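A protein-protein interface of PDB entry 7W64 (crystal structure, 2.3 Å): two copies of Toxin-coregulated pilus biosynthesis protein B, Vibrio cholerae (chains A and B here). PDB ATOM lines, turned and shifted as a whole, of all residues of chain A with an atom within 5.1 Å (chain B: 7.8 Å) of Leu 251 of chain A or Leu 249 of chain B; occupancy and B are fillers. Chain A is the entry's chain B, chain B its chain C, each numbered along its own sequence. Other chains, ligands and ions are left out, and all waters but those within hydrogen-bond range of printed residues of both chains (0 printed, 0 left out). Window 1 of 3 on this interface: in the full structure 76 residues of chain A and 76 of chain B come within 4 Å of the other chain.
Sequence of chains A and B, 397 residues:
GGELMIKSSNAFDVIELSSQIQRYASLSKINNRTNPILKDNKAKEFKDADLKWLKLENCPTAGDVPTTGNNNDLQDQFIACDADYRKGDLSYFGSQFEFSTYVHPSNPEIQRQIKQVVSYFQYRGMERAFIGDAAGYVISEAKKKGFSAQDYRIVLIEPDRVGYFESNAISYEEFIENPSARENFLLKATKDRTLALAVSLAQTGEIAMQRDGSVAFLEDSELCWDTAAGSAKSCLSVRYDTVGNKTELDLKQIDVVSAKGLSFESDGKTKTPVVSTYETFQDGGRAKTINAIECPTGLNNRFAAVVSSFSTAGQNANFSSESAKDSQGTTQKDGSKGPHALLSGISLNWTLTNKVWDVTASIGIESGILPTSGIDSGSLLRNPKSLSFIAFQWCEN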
ATOM      1  N   LEU A 236      -0.630  17.556 -26.952  1.00  0.00           N
ATOM      2  CA  LEU A 236      -0.114  18.066 -28.209  1.00  0.00           C
ATOM      3  C   LEU A 236      -1.088  17.672 -29.311  1.00  0.00           C
ATOM      4  O   LEU A 236      -1.960  16.825 -29.111  1.00  0.00           O
ATOM      5  CB  LEU A 236       1.281  17.525 -28.498  1.00  0.00           C
ATOM      6  CG  LEU A 236       1.404  16.019 -28.503  1.00  0.00           C
ATOM      7  CD1 LEU A 236       1.268  15.497 -29.942  1.00  0.00           C
ATOM      8  CD2 LEU A 236       2.709  15.615 -27.869  1.00  0.00           C
ATOM      9  N   LEU A 249       2.664  21.308 -35.788  1.00  0.00           N
ATOM     10  CA  LEU A 249       2.740  20.378 -34.666  1.00  0.00           C
ATOM     11  C   LEU A 249       2.848  21.247 -33.429  1.00  0.00           C
ATOM     12  O   LEU A 249       3.895  21.840 -33.161  1.00  0.00           O
ATOM     13  CB  LEU A 249       3.919  19.425 -34.794  1.00  0.00           C
ATOM     14  CG  LEU A 249       4.145  18.582 -33.534  1.00  0.00           C
ATOM     15  CD1 LEU A 249       2.909  17.777 -33.228  1.00  0.00           C
ATOM     16  CD2 LEU A 249       5.335  17.656 -33.721  1.00  0.00           C
ATOM     17  N   ASP A 250       1.744  21.359 -32.702  1.00  0.00           N
ATOM     18  CA  ASP A 250       1.619  22.297 -31.601  1.00  0.00           C
ATOM     19  C   ASP A 250       2.027  21.606 -30.310  1.00  0.00           C
ATOM     20  O   ASP A 250       1.304  20.729 -29.799  1.00  0.00           O
ATOM     21  CB  ASP A 250       0.195  22.829 -31.524  1.00  0.00           C
ATOM     22  CG  ASP A 250       0.004  23.790 -30.393  1.00  0.00           C
ATOM     23  OD1 ASP A 250       1.009  24.188 -29.747  1.00  0.00           O
ATOM     24  OD2 ASP A 250      -1.152  24.153 -30.140  1.00  0.00           O
ATOM     25  N   LEU A 251       3.204  21.987 -29.806  1.00  0.00           N
ATOM     26  CA  LEU A 251       3.748  21.517 -28.540  1.00  0.00           C
ATOM     27  C   LEU A 251       3.703  22.587 -27.459  1.00  0.00           C
ATOM     28  O   LEU A 251       4.331  22.423 -26.409  1.00  0.00           O
ATOM     29  CB  LEU A 251       5.193  21.017 -28.731  1.00  0.00           C
ATOM     30  CG  LEU A 251       5.377  20.015 -29.872  1.00  0.00           C
ATOM     31  CD1 LEU A 251       6.856  19.664 -30.122  1.00  0.00           C
ATOM     32  CD2 LEU A 251       4.553  18.738 -29.593  1.00  0.00           C
ATOM     33  N   LYS A 252       2.990  23.686 -27.690  1.00  0.00           N
ATOM     34  CA  LYS A 252       3.105  24.804 -26.764  1.00  0.00           C
ATOM     35  C   LYS A 252       2.447  24.540 -25.414  1.00  0.00           C
ATOM     36  O   LYS A 252       2.707  25.283 -24.465  1.00  0.00           O
ATOM     37  CB  LYS A 252       2.548  26.080 -27.414  1.00  0.00           C
ATOM     38  CG  LYS A 252       3.440  26.592 -28.549  1.00  0.00           C
ATOM     39  CD  LYS A 252       3.053  28.002 -28.998  1.00  0.00           C
ATOM     40  CE  LYS A 252       1.706  27.994 -29.671  1.00  0.00           C
ATOM     41  NZ  LYS A 252       1.746  27.150 -30.893  1.00  0.00           N
ATOM     42  N   GLN A 253       1.636  23.494 -25.274  1.00  0.00           N
ATOM     43  CA  GLN A 253       1.115  23.215 -23.939  1.00  0.00           C
ATOM     44  C   GLN A 253       2.164  22.637 -23.006  1.00  0.00           C
ATOM     45  O   GLN A 253       2.042  22.811 -21.792  1.00  0.00           O
ATOM     46  CB  GLN A 253      -0.060  22.248 -24.006  1.00  0.00           C
ATOM     47  CG  GLN A 253      -1.425  22.899 -24.083  1.00  0.00           C
ATOM     48  CD  GLN A 253      -2.539  21.868 -24.196  1.00  0.00           C
ATOM     49  OE1 GLN A 253      -2.671  20.999 -23.326  1.00  0.00           O
ATOM     50  NE2 GLN A 253      -3.381  22.000 -25.216  1.00  0.00           N
ATOM     51  N   ILE A 254       3.233  22.055 -23.538  1.00  0.00           N
ATOM     52  CA  ILE A 254       4.289  21.463 -22.730  1.00  0.00           C
ATOM     53  C   ILE A 254       5.364  22.510 -22.483  1.00  0.00           C
ATOM     54  O   ILE A 254       5.654  23.339 -23.360  1.00  0.00           O
ATOM     55  CB  ILE A 254       4.873  20.232 -23.437  1.00  0.00           C
ATOM     56  CG1 ILE A 254       3.759  19.366 -24.017  1.00  0.00           C
ATOM     57  CG2 ILE A 254       5.716  19.403 -22.462  1.00  0.00           C
ATOM     58  CD1 ILE A 254       4.276  18.155 -24.748  1.00  0.00           C
ATOM     59  N   VAL A 256       8.801  22.333 -21.832  1.00  0.00           N
ATOM     60  CA  VAL A 256      10.056  22.186 -22.548  1.00  0.00           C
ATOM     61  C   VAL A 256       9.996  20.950 -23.438  1.00  0.00           C
ATOM     62  O   VAL A 256       9.616  19.871 -22.976  1.00  0.00           O
ATOM     63  CB  VAL A 256      11.260  22.076 -21.586  1.00  0.00           C
ATOM     64  CG1 VAL A 256      12.548  21.790 -22.381  1.00  0.00           C
ATOM     65  CG2 VAL A 256      11.419  23.319 -20.716  1.00  0.00           C
ATOM     66  N   VAL A 257      10.386  21.112 -24.708  1.00  0.00           N
ATOM     67  CA  VAL A 257      10.685  20.012 -25.623  1.00  0.00           C
ATOM     68  C   VAL A 257      12.180  19.725 -25.516  1.00  0.00           C
ATOM     69  O   VAL A 257      13.005  20.639 -25.620  1.00  0.00           O
ATOM     70  CB  VAL A 257      10.289  20.357 -27.068  1.00  0.00           C
ATOM     71  CG1 VAL A 257      10.656  19.212 -28.034  1.00  0.00           C
ATOM     72  CG2 VAL A 257       8.811  20.693 -27.155  1.00  0.00           C
ATOM     73  N   SER A 258      12.518  18.479 -25.215  1.00  0.00           N
ATOM     74  CA  SER A 258      13.877  18.039 -24.922  1.00  0.00           C
ATOM     75  C   SER A 258      14.330  17.034 -25.977  1.00  0.00           C
ATOM     76  O   SER A 258      13.924  15.873 -25.965  1.00  0.00           O
ATOM     77  CB  SER A 258      13.929  17.441 -23.516  1.00  0.00           C
ATOM     78  OG  SER A 258      15.173  16.819 -23.267  1.00  0.00           O
ATOM     79  N   PRO B 105      -3.185  27.559 -25.301  1.00  0.00           N
ATOM     80  CA  PRO B 105      -2.156  28.162 -26.165  1.00  0.00           C
ATOM     81  C   PRO B 105      -2.583  28.353 -27.607  1.00  0.00           C
ATOM     82  O   PRO B 105      -1.884  29.067 -28.346  1.00  0.00           O
ATOM     83  CB  PRO B 105      -0.986  27.168 -26.075  1.00  0.00           C
ATOM     84  CG  PRO B 105      -1.216  26.404 -24.827  1.00  0.00           C
ATOM     85  CD  PRO B 105      -2.709  26.321 -24.659  1.00  0.00           C
ATOM     86  N   SER B 106      -3.689  27.749 -28.038  1.00  0.00           N
ATOM     87  CA  SER B 106      -4.095  27.861 -29.432  1.00  0.00           C
ATOM     88  C   SER B 106      -5.601  28.023 -29.610  1.00  0.00           C
ATOM     89  O   SER B 106      -6.083  27.972 -30.751  1.00  0.00           O
ATOM     90  CB  SER B 106      -3.598  26.648 -30.233  1.00  0.00           C
ATOM     91  OG  SER B 106      -2.178  26.619 -30.286  1.00  0.00           O
ATOM     92  N   LEU B 236       8.782   8.074 -26.537  1.00  0.00           N
ATOM     93  CA  LEU B 236       8.728   9.429 -26.023  1.00  0.00           C
ATOM     94  C   LEU B 236       7.651   9.466 -24.956  1.00  0.00           C
ATOM     95  O   LEU B 236       6.838   8.549 -24.837  1.00  0.00           O
ATOM     96  CB  LEU B 236       8.484  10.458 -27.140  1.00  0.00           C
ATOM     97  CG  LEU B 236       7.312  10.227 -28.093  1.00  0.00           C
ATOM     98  CD1 LEU B 236       6.038  10.930 -27.661  1.00  0.00           C
ATOM     99  CD2 LEU B 236       7.709  10.671 -29.471  1.00  0.00           C
ATOM    100  N   SER B 237       7.686  10.510 -24.141  1.00  0.00           N
ATOM    101  CA  SER B 237       6.742  10.626 -23.049  1.00  0.00           C
ATOM    102  C   SER B 237       6.687  12.079 -22.618  1.00  0.00           C
ATOM    103  O   SER B 237       7.587  12.869 -22.917  1.00  0.00           O
ATOM    104  CB  SER B 237       7.145   9.753 -21.862  1.00  0.00           C
ATOM    105  OG  SER B 237       8.372  10.200 -21.334  1.00  0.00           O
ATOM    106  N   VAL B 238       5.638  12.407 -21.868  1.00  0.00           N
ATOM    107  CA  VAL B 238       5.469  13.732 -21.295  1.00  0.00           C
ATOM    108  C   VAL B 238       5.519  13.557 -19.793  1.00  0.00           C
ATOM    109  O   VAL B 238       4.602  12.993 -19.190  1.00  0.00           O
ATOM    110  CB  VAL B 238       4.173  14.411 -21.748  1.00  0.00           C
ATOM    111  CG1 VAL B 238       3.970  15.728 -20.998  1.00  0.00           C
ATOM    112  CG2 VAL B 238       4.233  14.677 -23.254  1.00  0.00           C
ATOM    113  N   ARG B 239       6.588  14.032 -19.194  1.00  0.00           N
ATOM    114  CA  ARG B 239       6.822  13.917 -17.772  1.00  0.00           C
ATOM    115  C   ARG B 239       6.543  15.252 -17.096  1.00  0.00           C
ATOM    116  O   ARG B 239       6.725  16.318 -17.687  1.00  0.00           O
ATOM    117  CB  ARG B 239       8.280  13.524 -17.546  1.00  0.00           C
ATOM    118  CG  ARG B 239       8.749  13.608 -16.108  1.00  0.00           C
ATOM    119  CD  ARG B 239      10.245  13.365 -16.034  1.00  0.00           C
ATOM    120  NE  ARG B 239      10.655  12.060 -16.548  1.00  0.00           N
ATOM    121  CZ  ARG B 239      11.919  11.735 -16.816  1.00  0.00           C
ATOM    122  NH1 ARG B 239      12.892  12.628 -16.621  1.00  0.00           N
ATOM    123  NH2 ARG B 239      12.218  10.524 -17.285  1.00  0.00           N
ATOM    124  N   TYR B 240       6.185  15.186 -15.826  1.00  0.00           N
ATOM    125  CA  TYR B 240       6.027  16.363 -14.993  1.00  0.00           C
ATOM    126  C   TYR B 240       7.026  16.256 -13.847  1.00  0.00           C
ATOM    127  O   TYR B 240       7.157  15.195 -13.237  1.00  0.00           O
ATOM    128  CB  TYR B 240       4.584  16.470 -14.498  1.00  0.00           C
ATOM    129  CG  TYR B 240       4.427  17.564 -13.510  1.00  0.00           C
ATOM    130  CD1 TYR B 240       4.703  17.306 -12.192  1.00  0.00           C
ATOM    131  CD2 TYR B 240       4.040  18.857 -13.870  1.00  0.00           C
ATOM    132  CE1 TYR B 240       4.616  18.270 -11.241  1.00  0.00           C
ATOM    133  CE2 TYR B 240       3.934  19.864 -12.891  1.00  0.00           C
ATOM    134  CZ  TYR B 240       4.229  19.551 -11.575  1.00  0.00           C
ATOM    135  OH  TYR B 240       4.155  20.478 -10.553  1.00  0.00           O
ATOM    136  N   LYS B 246       7.257  21.929 -13.741  1.00  0.00           N
ATOM    137  CA  LYS B 246       7.282  22.074 -15.191  1.00  0.00           C
ATOM    138  C   LYS B 246       7.029  20.724 -15.857  1.00  0.00           C
ATOM    139  O   LYS B 246       7.391  19.677 -15.321  1.00  0.00           O
ATOM    140  CB  LYS B 246       8.635  22.623 -15.672  1.00  0.00           C
ATOM    141  CG  LYS B 246       8.923  24.072 -15.279  1.00  0.00           C
ATOM    142  CD  LYS B 246       7.885  25.080 -15.753  1.00  0.00           C
ATOM    143  CE  LYS B 246       8.074  26.384 -14.981  1.00  0.00           C
ATOM    144  NZ  LYS B 246       7.804  27.579 -15.815  1.00  0.00           N
ATOM    145  N   THR B 247       6.422  20.754 -17.040  1.00  0.00           N
ATOM    146  CA  THR B 247       6.281  19.561 -17.867  1.00  0.00           C
ATOM    147  C   THR B 247       7.333  19.533 -18.980  1.00  0.00           C
ATOM    148  O   THR B 247       7.743  20.575 -19.504  1.00  0.00           O
ATOM    149  CB  THR B 247       4.895  19.485 -18.499  1.00  0.00           C
ATOM    150  OG1 THR B 247       4.718  20.603 -19.370  1.00  0.00           O
ATOM    151  CG2 THR B 247       3.776  19.486 -17.401  1.00  0.00           C
ATOM    152  N   GLU B 248       7.745  18.316 -19.352  1.00  0.00           N
ATOM    153  CA  GLU B 248       8.789  18.070 -20.344  1.00  0.00           C
ATOM    154  C   GLU B 248       8.299  17.056 -21.373  1.00  0.00           C
ATOM    155  O   GLU B 248       7.795  15.998 -21.004  1.00  0.00           O
ATOM    156  CB  GLU B 248      10.086  17.545 -19.686  1.00  0.00           C
ATOM    157  CG  GLU B 248      11.157  17.120 -20.744  1.00  0.00           C
ATOM    158  CD  GLU B 248      12.526  16.700 -20.168  1.00  0.00           C
ATOM    159  OE1 GLU B 248      13.251  17.580 -19.646  1.00  0.00           O
ATOM    160  OE2 GLU B 248      12.899  15.509 -20.280  1.00  0.00           O
ATOM    161  N   LEU B 249       8.408  17.375 -22.659  1.00  0.00           N
ATOM    162  CA  LEU B 249       8.238  16.358 -23.692  1.00  0.00           C
ATOM    163  C   LEU B 249       9.599  15.723 -23.944  1.00  0.00           C
ATOM    164  O   LEU B 249      10.488  16.343 -24.548  1.00  0.00           O
ATOM    165  CB  LEU B 249       7.640  16.948 -24.962  1.00  0.00           C
ATOM    166  CG  LEU B 249       7.580  16.043 -26.188  1.00  0.00           C
ATOM    167  CD1 LEU B 249       6.760  14.835 -25.922  1.00  0.00           C
ATOM    168  CD2 LEU B 249       7.037  16.806 -27.382  1.00  0.00           C
ATOM    169  N   ASP B 250       9.768  14.500 -23.467  1.00  0.00           N
ATOM    170  CA  ASP B 250      11.059  13.830 -23.488  1.00  0.00           C
ATOM    171  C   ASP B 250      11.178  13.064 -24.797  1.00  0.00           C
ATOM    172  O   ASP B 250      10.541  12.014 -24.972  1.00  0.00           O
ATOM    173  CB  ASP B 250      11.199  12.882 -22.301  1.00  0.00           C
ATOM    174  CG  ASP B 250      12.542  12.182 -22.275  1.00  0.00           C
ATOM    175  OD1 ASP B 250      13.411  12.542 -23.083  1.00  0.00           O
ATOM    176  OD2 ASP B 250      12.740  11.288 -21.435  1.00  0.00           O
ATOM    177  N   LEU B 251      11.998  13.587 -25.707  1.00  0.00           N
ATOM    178  CA  LEU B 251      12.306  12.918 -26.962  1.00  0.00           C
ATOM    179  C   LEU B 251      13.711  12.337 -26.953  1.00  0.00           C
ATOM    180  O   LEU B 251      14.183  11.862 -27.989  1.00  0.00           O
ATOM    181  CB  LEU B 251      12.140  13.881 -28.145  1.00  0.00           C
ATOM    182  CG  LEU B 251      10.806  14.624 -28.223  1.00  0.00           C
ATOM    183  CD1 LEU B 251      10.814  15.701 -29.300  1.00  0.00           C
ATOM    184  CD2 LEU B 251       9.768  13.605 -28.585  1.00  0.00           C
ATOM    185  N   LYS B 252      14.361  12.320 -25.792  1.00  0.00           N
ATOM    186  CA  LYS B 252      15.774  12.003 -25.720  1.00  0.00           C
ATOM    187  C   LYS B 252      16.073  10.540 -25.986  1.00  0.00           C
ATOM    188  O   LYS B 252      17.246  10.196 -26.147  1.00  0.00           O
ATOM    189  CB  LYS B 252      16.332  12.401 -24.354  1.00  0.00           C
ATOM    190  CG  LYS B 252      16.350  13.906 -24.126  1.00  0.00           C
ATOM    191  CD  LYS B 252      17.240  14.258 -22.944  1.00  0.00           C
ATOM    192  CE  LYS B 252      16.684  13.772 -21.645  1.00  0.00           C
ATOM    193  NZ  LYS B 252      15.394  14.434 -21.349  1.00  0.00           N
ATOM    194  N   VAL B 257      15.636  14.289 -33.715  1.00  0.00           N
ATOM    195  CA  VAL B 257      14.358  14.854 -34.101  1.00  0.00           C
ATOM    196  C   VAL B 257      14.574  15.674 -35.362  1.00  0.00           C
ATOM    197  O   VAL B 257      15.313  16.656 -35.343  1.00  0.00           O
ATOM    198  CB  VAL B 257      13.786  15.734 -32.985  1.00  0.00           C
ATOM    199  CG1 VAL B 257      12.511  16.373 -33.464  1.00  0.00           C
ATOM    200  CG2 VAL B 257      13.596  14.917 -31.684  1.00  0.00           C
ATOM    201  N   LEU B 262      10.556  25.141 -37.541  1.00  0.00           N
ATOM    202  CA  LEU B 262      10.688  24.972 -36.102  1.00  0.00           C
ATOM    203  C   LEU B 262      10.661  26.340 -35.440  1.00  0.00           C
ATOM    204  O   LEU B 262      11.428  27.232 -35.832  1.00  0.00           O
ATOM    205  CB  LEU B 262      12.000  24.247 -35.760  1.00  0.00           C
ATOM    206  CG  LEU B 262      12.400  24.082 -34.290  1.00  0.00           C
ATOM    207  CD1 LEU B 262      11.415  23.197 -33.514  1.00  0.00           C
ATOM    208  CD2 LEU B 262      13.819  23.522 -34.181  1.00  0.00           C
ATOM    209  N   SER B 263       9.811  26.490 -34.427  1.00  0.00           N
ATOM    210  CA  SER B 263       9.721  27.710 -33.643  1.00  0.00           C
ATOM    211  C   SER B 263       9.703  27.329 -32.172  1.00  0.00           C
ATOM    212  O   SER B 263       9.406  26.197 -31.808  1.00  0.00           O
ATOM    213  CB  SER B 263       8.484  28.570 -34.005  1.00  0.00           C
ATOM    214  OG  SER B 263       7.270  27.981 -33.518  1.00  0.00           O
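The side-chain carboxylate (OD2) of Asp 250 of chain A is in hydrogen-bond range of the side-chain hydroxyl (OG) of Ser 106 of chain B, 2.7 Å away. The backbone NH of Val 256 of chain A is in hydrogen-bond range of the backbone carbonyl oxygen of Thr 247 of chain B (3.1 Å). The backbone carbonyl oxygen (O) of Val 256 of chain A sits at hydrogen-bond distance from the backbone NH (N) of Leu 249 of chain B (2.8 Å). N of Ser 258 of chain A is in hydrogen-bond range of O of Leu 249 of chain B (3.0 Å). O of Ser 258 of chain A lies within hydrogen-bond range of N of Leu 251 of chain B, at 3.0 Å. The side-chain hydroxyl of Ser 258 of chain A is in hydrogen-bond range of the side-chain amino group of Lys 252 of chain B (3.1 Å).
The side-chain amino group (NZ) of Lys 252 of chain A lies within salt-bridge range of the side-chain carboxylate (OD1) of Asp 250 of chain A (3.3 Å). O of Arg 239 of chain B lies within hydrogen-bond range of N of Glu 248 of chain B, 2.8 Å away. OE2 of Glu 248 of chain B lies within salt-bridge range of NZ of Lys 252 of chain B (2.9 Å). The side-chain carboxylate of Asp 250 of chain B lies within salt-bridge range of the side-chain amino group of Lys 252 of chain B (3.2 Å).
Leu 251 of chain A touches Leu 249 of chain B, but with the chains exchanged Leu 249 of chain A does not touch Leu 251 of chain B (7.3 Å). Val 257 of chain A touches Leu 249 of chain B, but with the chains exchanged Leu 249 of chain A does not touch Val 257 of chain B (7.3 Å). Val 257 of chain A touches Leu 251 of chain B, but with the chains exchanged Leu 251 of chain A does not touch Val 257 of chain B (7.3 Å). 6 positions are printed for both chains. Of the 17 pairs that touch across the chains among the printed residues, none has its exchanged pair printed and touching as well.
Printed residues of chain A that touch a printed residue of chain B: Asp 250, Leu 251, Lys 252, Gln 253, Ile 254, Val 256, Val 257 and Ser 258. Printed residues of chain B that touch a printed residue of chain A: Pro 105, Ser 106, Val 238, Thr 247, Glu 248, Leu 249, Leu 251 and Lys 252. Hydrophobic or aromatic side chains of chain B within 4 Å of the printed part of chain A: Pro 105, Val 238, Leu 249 and Leu 251.
Among the printed residues, merely in contact across the chains: Val 256 of chain A with Glu 248 of chain B, Ile 254 of chain A with Leu 249 of chain B, Ile 254 of chain A with Thr 247 of chain B, Gln 253 of chain A with Pro 105 of chain B, Ile 254 of chain A with Glu 248 of chain B, Ser 258 of chain A with Glu 248 of chain B, Val 257 of chain A with Leu 251 of chain B, Ile 254 of chain A with Val 238 of chain B, Val 257 of chain A with Leu 249 of chain B, Leu 251 of chain A with Leu 249 of chain B and Lys 252 of chain A with Pro 105 of chain B.
Printed residues of chain B within 4 Å of Lys 252 of chain A: Pro 105. Printed residues of chain A within 4 Å of Ser 106 of chain B: Asp 250 (2.7 Å). Ser 237 of chain B touches none of the printed residues of chain A. Of the printed residues of chain A, Val 238 of chain B touches Ile 254. Leu 249 of chain B touches just these residues of chain A: Leu 251 (3.8 Å), Ile 254 (3.4 Å), Val 256 (2.8 Å), Val 257 (3.8 Å) and Ser 258 (3.0 Å). Of the printed residues of chain A, Leu 251 of chain B touches Val 257 (3.7 Å) and Ser 258 (3.0 Å). Val 257 of chain B touches none of the printed residues of chain A. The nearest printed residue of chain A that does not touch Lys 252 of chain B is Val 257 of chain A (7.3 Å).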
